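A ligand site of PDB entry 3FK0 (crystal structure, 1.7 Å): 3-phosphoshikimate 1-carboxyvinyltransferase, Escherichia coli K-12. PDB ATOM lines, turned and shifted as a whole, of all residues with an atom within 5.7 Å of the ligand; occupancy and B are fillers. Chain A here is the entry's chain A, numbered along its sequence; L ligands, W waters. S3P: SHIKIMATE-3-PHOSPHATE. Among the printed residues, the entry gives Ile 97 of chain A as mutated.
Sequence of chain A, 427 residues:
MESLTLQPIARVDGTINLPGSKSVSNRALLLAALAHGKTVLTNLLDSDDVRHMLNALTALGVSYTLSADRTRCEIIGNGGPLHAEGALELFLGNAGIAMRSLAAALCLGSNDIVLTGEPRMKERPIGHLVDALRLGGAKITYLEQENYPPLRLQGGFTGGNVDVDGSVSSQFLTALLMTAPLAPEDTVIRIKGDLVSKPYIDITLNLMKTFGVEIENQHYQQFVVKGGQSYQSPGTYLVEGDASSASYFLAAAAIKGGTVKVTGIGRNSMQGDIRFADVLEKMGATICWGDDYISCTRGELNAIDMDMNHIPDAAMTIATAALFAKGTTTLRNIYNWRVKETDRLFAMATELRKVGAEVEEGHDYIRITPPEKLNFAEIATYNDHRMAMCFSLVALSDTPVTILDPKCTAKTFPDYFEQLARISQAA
The side-chain hydroxyl (OG) of Ser 197 lies within hydrogen-bond range of an oxygen (O7) of the ligand (2.6 Å).
N of Ser 170 sits at hydrogen-bond distance from O6 of the ligand (2.8 Å).
An oxygen (O6) of the ligand is in hydrogen-bond range of the side-chain hydroxyl (OG) of Ser 170, 2.6 Å away.
NH1 of Arg 27 is in salt-bridge range of O4 of the ligand, 2.6 Å away.
The side-chain hydroxyl of Ser 23 lies within hydrogen-bond range of an oxygen (O5) of the ligand (2.6 Å).
O7 of the ligand lies within salt-bridge range of NZ of Lys 340.
An oxygen (O8) of the ligand sits at hydrogen-bond distance from the side-chain hydroxyl of Ser 169 (2.7 Å).
OD1 of Asp 313 lies within hydrogen-bond range of O3 of the ligand, 2.7 Å away.
An oxygen (O7) of the ligand is in hydrogen-bond range of the side-chain amide nitrogen (ND2) of Asn 336, 2.8 Å away.
An oxygen (O1) of the ligand sits at hydrogen-bond distance from the side-chain amide nitrogen (NE2) of Gln 171 (3.0 Å).
The side-chain amino group of Lys 22 sits at hydrogen-bond distance from an oxygen (O3) of the ligand, 3.1 Å away.
O of Ser 23 lies within hydrogen-bond range of NH2 of Arg 27.
The backbone carbonyl oxygen (O) of Tyr 200 is in hydrogen-bond range of the guanidinium group (NH1) of Arg 27 (3.4 Å).
The guanidinium group (NH1) of Arg 27 is in hydrogen-bond range of the side-chain hydroxyl (OG1) of Thr 174.
The side-chain hydroxyl of Thr 204 lies within hydrogen-bond range of the guanidinium group of Arg 27 (2.9 Å).
The side-chain hydroxyl (OG) of Ser 169 sits at hydrogen-bond distance from the backbone NH (N) of Gln 171.
The side-chain carboxylate of Asp 313 is in salt-bridge range of the guanidinium group of Arg 386 (3.7 Å).
The side-chain amide oxygen (OE1) of Gln 171 is in hydrogen-bond range of the backbone NH (N) of Ile 97.
The side-chain amide oxygen (OE1) of Gln 171 sits at hydrogen-bond distance from the guanidinium group (NH2) of Arg 100.
Merely in contact with the ligand: Ile 97 (3.4 Å) and Tyr 200 (3.2 Å).
Hydrophobic or aromatic side chains that line the ligand: Ile 97 and Tyr 200.
Water W1 bridges O8 of the ligand (2.5 Å) and O of Val 168 (2.9 Å).
Water W3 bridges O5 of the ligand (2.6 Å) and OG of Ser 23 (3.5 Å).
Water W5 lies within hydrogen-bond range of an oxygen (O4) of the ligand (2.8 Å), the side-chain hydroxyl of Thr 174 (2.8 Å), the side-chain hydroxyl of Ser 170 (3.0 Å) and the guanidinium group of Arg 27 (3.2 Å).
Water W2 lies within hydrogen-bond range of the side-chain amide nitrogen (NE2) of Gln 171 (2.8 Å), an oxygen (O8) of the ligand (3.0 Å) and the guanidinium group (NH2) of Arg 100 (3.1 Å).
Water W4 bridges the side-chain carboxylate (OE1) of Glu 341 (2.9 Å) and an oxygen (O3) of the ligand (3.2 Å).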
ATOM      1  N   LYS A  22       6.745   5.078 -15.562  1.00  0.00           N
ATOM      2  CA  LYS A  22       6.631   6.179 -14.598  1.00  0.00           C
ATOM      3  C   LYS A  22       5.816   5.713 -13.379  1.00  0.00           C
ATOM      4  O   LYS A  22       6.161   6.045 -12.235  1.00  0.00           O
ATOM      5  CB  LYS A  22       5.967   7.410 -15.253  1.00  0.00           C
ATOM      6  CG  LYS A  22       5.738   8.599 -14.284  1.00  0.00           C
ATOM      7  CD  LYS A  22       4.261   8.690 -13.852  1.00  0.00           C
ATOM      8  CE  LYS A  22       3.430   9.314 -14.982  1.00  0.00           C
ATOM      9  NZ  LYS A  22       1.971   9.179 -14.814  1.00  0.00           N
ATOM     10  N   SER A  23       4.759   4.946 -13.593  1.00  0.00           N
ATOM     11  CA  SER A  23       3.956   4.470 -12.468  1.00  0.00           C
ATOM     12  C   SER A  23       4.757   3.609 -11.509  1.00  0.00           C
ATOM     13  O   SER A  23       4.655   3.752 -10.303  1.00  0.00           O
ATOM     14  CB  SER A  23       2.745   3.661 -12.948  1.00  0.00           C
ATOM     15  OG  SER A  23       1.871   4.506 -13.681  1.00  0.00           O
ATOM     16  N   ARG A  27       6.491   4.756  -7.472  1.00  0.00           N
ATOM     17  CA  ARG A  27       6.056   3.915  -6.349  1.00  0.00           C
ATOM     18  C   ARG A  27       7.302   3.222  -5.773  1.00  0.00           C
ATOM     19  O   ARG A  27       7.500   3.162  -4.564  1.00  0.00           O
ATOM     20  CB  ARG A  27       5.091   2.851  -6.833  1.00  0.00           C
ATOM     21  CG  ARG A  27       3.676   3.330  -7.157  1.00  0.00           C
ATOM     22  CD  ARG A  27       2.912   2.170  -7.790  1.00  0.00           C
ATOM     23  NE  ARG A  27       1.468   2.393  -7.948  1.00  0.00           N
ATOM     24  CZ  ARG A  27       0.910   3.191  -8.850  1.00  0.00           C
ATOM     25  NH1 ARG A  27      -0.405   3.282  -8.904  1.00  0.00           N
ATOM     26  NH2 ARG A  27       1.645   3.904  -9.708  1.00  0.00           N
ATOM     27  N   ILE A  97       1.063  10.895  -9.071  1.00  0.00           N
ATOM     28  CA  ILE A  97       1.357   9.862  -8.091  1.00  0.00           C
ATOM     29  C   ILE A  97       2.259  10.393  -6.993  1.00  0.00           C
ATOM     30  O   ILE A  97       2.033  10.101  -5.825  1.00  0.00           O
ATOM     31  CB  ILE A  97       1.955   8.589  -8.775  1.00  0.00           C
ATOM     32  CG1 ILE A  97       0.809   7.632  -9.137  1.00  0.00           C
ATOM     33  CG2 ILE A  97       2.897   7.846  -7.829  1.00  0.00           C
ATOM     34  CD1 ILE A  97       0.095   7.056  -7.903  1.00  0.00           C
ATOM     35  N   ARG A 100      -0.003  12.579  -4.670  1.00  0.00           N
ATOM     36  CA  ARG A 100      -0.968  11.828  -3.879  1.00  0.00           C
ATOM     37  C   ARG A 100      -0.269  10.889  -2.892  1.00  0.00           C
ATOM     38  O   ARG A 100      -0.619  10.858  -1.716  1.00  0.00           O
ATOM     39  CB  ARG A 100      -1.931  11.059  -4.783  1.00  0.00           C
ATOM     40  CG  ARG A 100      -3.122  11.872  -5.311  1.00  0.00           C
ATOM     41  CD  ARG A 100      -2.685  13.015  -6.230  1.00  0.00           C
ATOM     42  NE  ARG A 100      -3.836  13.707  -6.847  1.00  0.00           N
ATOM     43  CZ  ARG A 100      -4.404  13.355  -8.002  1.00  0.00           C
ATOM     44  NH1 ARG A 100      -5.441  14.052  -8.464  1.00  0.00           N
ATOM     45  NH2 ARG A 100      -3.935  12.334  -8.704  1.00  0.00           N
ATOM     46  N   VAL A 168     -13.240   9.151  -8.610  1.00  0.00           N
ATOM     47  CA  VAL A 168     -12.538  10.156  -9.405  1.00  0.00           C
ATOM     48  C   VAL A 168     -11.097   9.749  -9.715  1.00  0.00           C
ATOM     49  O   VAL A 168     -10.619   9.928 -10.840  1.00  0.00           O
ATOM     50  CB  VAL A 168     -12.571  11.541  -8.696  1.00  0.00           C
ATOM     51  CG1 VAL A 168     -11.693  12.541  -9.445  1.00  0.00           C
ATOM     52  CG2 VAL A 168     -14.021  12.070  -8.661  1.00  0.00           C
ATOM     53  N   SER A 169     -10.386   9.217  -8.720  1.00  0.00           N
ATOM     54  CA  SER A 169      -9.025   8.771  -8.932  1.00  0.00           C
ATOM     55  C   SER A 169      -8.700   7.537  -8.100  1.00  0.00           C
ATOM     56  O   SER A 169      -9.091   7.425  -6.923  1.00  0.00           O
ATOM     57  CB  SER A 169      -8.005   9.873  -8.574  1.00  0.00           C
ATOM     58  OG  SER A 169      -6.664   9.459  -8.870  1.00  0.00           O
ATOM     59  N   SER A 170      -8.005   6.597  -8.717  1.00  0.00           N
ATOM     60  CA  SER A 170      -7.589   5.405  -8.015  1.00  0.00           C
ATOM     61  C   SER A 170      -6.340   5.792  -7.215  1.00  0.00           C
ATOM     62  O   SER A 170      -5.915   5.058  -6.331  1.00  0.00           O
ATOM     63  CB  SER A 170      -7.202   4.293  -9.007  1.00  0.00           C
ATOM     64  OG  SER A 170      -6.087   4.711  -9.796  1.00  0.00           O
ATOM     65  N   GLN A 171      -5.732   6.947  -7.519  1.00  0.00           N
ATOM     66  CA  GLN A 171      -4.506   7.343  -6.825  1.00  0.00           C
ATOM     67  C   GLN A 171      -4.690   7.610  -5.355  1.00  0.00           C
ATOM     68  O   GLN A 171      -3.738   7.509  -4.587  1.00  0.00           O
ATOM     69  CB  GLN A 171      -3.885   8.566  -7.494  1.00  0.00           C
ATOM     70  CG  GLN A 171      -3.347   8.262  -8.886  1.00  0.00           C
ATOM     71  CD  GLN A 171      -2.703   9.474  -9.522  1.00  0.00           C
ATOM     72  OE1 GLN A 171      -2.044  10.263  -8.846  1.00  0.00           O
ATOM     73  NE2 GLN A 171      -2.890   9.620 -10.826  1.00  0.00           N
ATOM     74  N   THR A 174      -4.431   4.202  -3.887  1.00  0.00           N
ATOM     75  CA  THR A 174      -3.028   3.773  -3.962  1.00  0.00           C
ATOM     76  C   THR A 174      -2.230   4.410  -2.824  1.00  0.00           C
ATOM     77  O   THR A 174      -1.476   3.737  -2.126  1.00  0.00           O
ATOM     78  CB  THR A 174      -2.405   4.191  -5.312  1.00  0.00           C
ATOM     79  OG1 THR A 174      -2.729   3.175  -6.289  1.00  0.00           O
ATOM     80  CG2 THR A 174      -0.899   4.352  -5.207  1.00  0.00           C
ATOM     81  N   VAL A 196     -12.470   3.743 -10.151  1.00  0.00           N
ATOM     82  CA  VAL A 196     -11.994   3.891 -11.520  1.00  0.00           C
ATOM     83  C   VAL A 196     -10.509   3.549 -11.612  1.00  0.00           C
ATOM     84  O   VAL A 196      -9.825   3.447 -10.591  1.00  0.00           O
ATOM     85  CB  VAL A 196     -12.190   5.352 -12.030  1.00  0.00           C
ATOM     86  CG1 VAL A 196     -13.684   5.688 -12.105  1.00  0.00           C
ATOM     87  CG2 VAL A 196     -11.477   6.317 -11.122  1.00  0.00           C
ATOM     88  N   SER A 197     -10.021   3.348 -12.842  1.00  0.00           N
ATOM     89  CA  SER A 197      -8.612   3.026 -13.081  1.00  0.00           C
ATOM     90  C   SER A 197      -8.148   1.882 -12.189  1.00  0.00           C
ATOM     91  O   SER A 197      -7.021   1.871 -11.685  1.00  0.00           O
ATOM     92  CB  SER A 197      -7.748   4.265 -12.816  1.00  0.00           C
ATOM     93  OG  SER A 197      -8.085   5.304 -13.718  1.00  0.00           O
ATOM     94  N   TYR A 200      -4.469   0.187 -11.862  1.00  0.00           N
ATOM     95  CA  TYR A 200      -3.369   0.851 -11.182  1.00  0.00           C
ATOM     96  C   TYR A 200      -3.287   0.400  -9.730  1.00  0.00           C
ATOM     97  O   TYR A 200      -2.219   0.456  -9.125  1.00  0.00           O
ATOM     98  CB  TYR A 200      -3.518   2.358 -11.277  1.00  0.00           C
ATOM     99  CG  TYR A 200      -3.178   2.848 -12.663  1.00  0.00           C
ATOM    100  CD1 TYR A 200      -4.178   3.117 -13.600  1.00  0.00           C
ATOM    101  CD2 TYR A 200      -1.843   3.012 -13.040  1.00  0.00           C
ATOM    102  CE1 TYR A 200      -3.857   3.541 -14.897  1.00  0.00           C
ATOM    103  CE2 TYR A 200      -1.498   3.448 -14.322  1.00  0.00           C
ATOM    104  CZ  TYR A 200      -2.512   3.708 -15.244  1.00  0.00           C
ATOM    105  OH  TYR A 200      -2.183   4.178 -16.494  1.00  0.00           O
ATOM    106  N   ILE A 203      -1.078  -2.453  -9.660  1.00  0.00           N
ATOM    107  CA  ILE A 203       0.339  -2.072  -9.748  1.00  0.00           C
ATOM    108  C   ILE A 203       0.823  -1.753  -8.327  1.00  0.00           C
ATOM    109  O   ILE A 203       1.907  -2.178  -7.921  1.00  0.00           O
ATOM    110  CB  ILE A 203       0.544  -0.810 -10.649  1.00  0.00           C
ATOM    111  CG1 ILE A 203       0.213  -1.132 -12.107  1.00  0.00           C
ATOM    112  CG2 ILE A 203       2.000  -0.296 -10.564  1.00  0.00           C
ATOM    113  CD1 ILE A 203       0.307   0.103 -13.029  1.00  0.00           C
ATOM    114  N   THR A 204       0.012  -1.031  -7.569  1.00  0.00           N
ATOM    115  CA  THR A 204       0.393  -0.658  -6.220  1.00  0.00           C
ATOM    116  C   THR A 204       0.611  -1.869  -5.330  1.00  0.00           C
ATOM    117  O   THR A 204       1.626  -1.998  -4.635  1.00  0.00           O
ATOM    118  CB  THR A 204      -0.660   0.251  -5.594  1.00  0.00           C
ATOM    119  OG1 THR A 204      -0.774   1.421  -6.418  1.00  0.00           O
ATOM    120  CG2 THR A 204      -0.264   0.652  -4.182  1.00  0.00           C
ATOM    121  N   PRO A 312      -7.148   4.542 -19.101  1.00  0.00           N
ATOM    122  CA  PRO A 312      -7.344   5.979 -19.358  1.00  0.00           C
ATOM    123  C   PRO A 312      -6.228   6.704 -20.104  1.00  0.00           C
ATOM    124  O   PRO A 312      -6.496   7.534 -20.974  1.00  0.00           O
ATOM    125  CB  PRO A 312      -7.608   6.546 -17.960  1.00  0.00           C
ATOM    126  CG  PRO A 312      -6.839   5.600 -17.053  1.00  0.00           C
ATOM    127  CD  PRO A 312      -7.150   4.247 -17.660  1.00  0.00           C
ATOM    128  N   ASP A 313      -4.975   6.375 -19.792  1.00  0.00           N
ATOM    129  CA  ASP A 313      -3.884   7.061 -20.479  1.00  0.00           C
ATOM    130  C   ASP A 313      -3.689   6.562 -21.903  1.00  0.00           C
ATOM    131  O   ASP A 313      -3.756   7.340 -22.863  1.00  0.00           O
ATOM    132  CB  ASP A 313      -2.570   6.916 -19.694  1.00  0.00           C
ATOM    133  CG  ASP A 313      -2.539   7.735 -18.427  1.00  0.00           C
ATOM    134  OD1 ASP A 313      -1.548   7.595 -17.682  1.00  0.00           O
ATOM    135  OD2 ASP A 313      -3.470   8.542 -18.194  1.00  0.00           O
ATOM    136  N   ASN A 336     -12.531  10.976 -15.863  1.00  0.00           N
ATOM    137  CA  ASN A 336     -11.369  11.587 -15.246  1.00  0.00           C
ATOM    138  C   ASN A 336     -10.264  12.126 -16.139  1.00  0.00           C
ATOM    139  O   ASN A 336      -9.260  12.681 -15.655  1.00  0.00           O
ATOM    140  CB  ASN A 336     -10.827  10.724 -14.076  1.00  0.00           C
ATOM    141  CG  ASN A 336     -10.054   9.519 -14.526  1.00  0.00           C
ATOM    142  OD1 ASN A 336      -9.738   9.335 -15.699  1.00  0.00           O
ATOM    143  ND2 ASN A 336      -9.721   8.664 -13.548  1.00  0.00           N
ATOM    144  N   LYS A 340      -6.796  15.441 -15.197  1.00  0.00           N
ATOM    145  CA  LYS A 340      -5.416  14.999 -15.286  1.00  0.00           C
ATOM    146  C   LYS A 340      -4.493  16.135 -15.705  1.00  0.00           C
ATOM    147  O   LYS A 340      -4.751  17.279 -15.344  1.00  0.00           O
ATOM    148  CB  LYS A 340      -5.336  13.800 -16.235  1.00  0.00           C
ATOM    149  CG  LYS A 340      -5.979  12.582 -15.575  1.00  0.00           C
ATOM    150  CD  LYS A 340      -6.007  11.393 -16.462  1.00  0.00           C
ATOM    151  CE  LYS A 340      -6.779  10.223 -15.847  1.00  0.00           C
ATOM    152  NZ  LYS A 340      -6.178   9.740 -14.612  1.00  0.00           N
ATOM    153  N   GLU A 341      -3.412  15.843 -16.449  1.00  0.00           N
ATOM    154  CA  GLU A 341      -2.451  16.880 -16.848  1.00  0.00           C
ATOM    155  C   GLU A 341      -3.105  18.144 -17.409  1.00  0.00           C
ATOM    156  O   GLU A 341      -2.569  19.235 -17.280  1.00  0.00           O
ATOM    157  CB  GLU A 341      -1.408  16.318 -17.814  1.00  0.00           C
ATOM    158  CG  GLU A 341      -0.284  15.524 -17.106  1.00  0.00           C
ATOM    159  CD  GLU A 341      -0.665  14.100 -16.713  1.00  0.00           C
ATOM    160  OE1 GLU A 341      -1.872  13.785 -16.544  1.00  0.00           O
ATOM    161  OE2 GLU A 341       0.264  13.272 -16.555  1.00  0.00           O
ATOM    162  N   ARG A 344      -8.315  16.582 -20.584  1.00  0.00           N
ATOM    163  CA  ARG A 344      -8.061  15.858 -21.831  1.00  0.00           C
ATOM    164  C   ARG A 344      -9.226  15.674 -22.774  1.00  0.00           C
ATOM    165  O   ARG A 344      -9.018  15.507 -23.974  1.00  0.00           O
ATOM    166  CB  ARG A 344      -7.413  14.506 -21.505  1.00  0.00           C
ATOM    167  CG  ARG A 344      -5.990  14.730 -21.029  1.00  0.00           C
ATOM    168  CD  ARG A 344      -5.416  13.527 -20.299  1.00  0.00           C
ATOM    169  NE  ARG A 344      -3.960  13.654 -20.251  1.00  0.00           N
ATOM    170  CZ  ARG A 344      -3.158  12.775 -19.668  1.00  0.00           C
ATOM    171  NH1 ARG A 344      -1.840  12.962 -19.699  1.00  0.00           N
ATOM    172  NH2 ARG A 344      -3.675  11.709 -19.054  1.00  0.00           N
ATOM    173  N   ARG A 386       1.173  13.754 -23.105  1.00  0.00           N
ATOM    174  CA  ARG A 386       0.412  12.876 -23.983  1.00  0.00           C
ATOM    175  C   ARG A 386      -0.290  13.548 -25.134  1.00  0.00           C
ATOM    176  O   ARG A 386      -0.592  12.898 -26.131  1.00  0.00           O
ATOM    177  CB  ARG A 386      -0.592  12.047 -23.183  1.00  0.00           C
ATOM    178  CG  ARG A 386       0.112  11.188 -22.117  1.00  0.00           C
ATOM    179  CD  ARG A 386      -0.751  10.011 -21.639  1.00  0.00           C
ATOM    180  NE  ARG A 386      -0.079   9.424 -20.482  1.00  0.00           N
ATOM    181  CZ  ARG A 386       1.052   8.721 -20.549  1.00  0.00           C
ATOM    182  NH1 ARG A 386       1.601   8.262 -19.423  1.00  0.00           N
ATOM    183  NH2 ARG A 386       1.595   8.419 -21.719  1.00  0.00           N
HETATM  184  C1  S3P L   1      -1.583   6.379 -12.436  1.00  0.00           C
HETATM  185  C2  S3P L   1      -2.987   6.228 -12.439  1.00  0.00           C
HETATM  186  C3  S3P L   1      -3.880   6.998 -13.410  1.00  0.00           C
HETATM  187  C4  S3P L   1      -3.043   7.560 -14.611  1.00  0.00           C
HETATM  188  C5  S3P L   1      -1.769   8.257 -14.142  1.00  0.00           C
HETATM  189  C6  S3P L   1      -0.915   7.250 -13.362  1.00  0.00           C
HETATM  190  C7  S3P L   1      -0.787   5.608 -11.432  1.00  0.00           C
HETATM  191  O1  S3P L   1      -4.695   8.061 -12.620  1.00  0.00           O
HETATM  192  O2  S3P L   1      -3.879   8.426 -15.408  1.00  0.00           O
HETATM  193  O3  S3P L   1      -1.042   8.748 -15.253  1.00  0.00           O
HETATM  194  O4  S3P L   1      -1.382   5.193 -10.415  1.00  0.00           O
HETATM  195  O5  S3P L   1       0.407   5.387 -11.682  1.00  0.00           O
HETATM  196  P1  S3P L   1      -6.339   7.959 -12.092  1.00  0.00           P
HETATM  197  O6  S3P L   1      -6.479   6.907 -11.099  1.00  0.00           O
HETATM  198  O7  S3P L   1      -7.139   7.640 -13.306  1.00  0.00           O
HETATM  199  O8  S3P L   1      -6.719   9.246 -11.523  1.00  0.00           O
HETATM  200  O   HOH W   1      -8.174  11.298 -11.743  1.00  0.00           O
HETATM  201  O   HOH W   2      -4.804  11.547 -11.622  1.00  0.00           O
HETATM  202  O   HOH W   3       2.118   7.403 -11.799  1.00  0.00           O
HETATM  203  O   HOH W   4      -2.708  11.452 -15.120  1.00  0.00           O
HETATM  204  O   HOH W   5      -3.367   4.531  -8.616  1.00  0.00           O
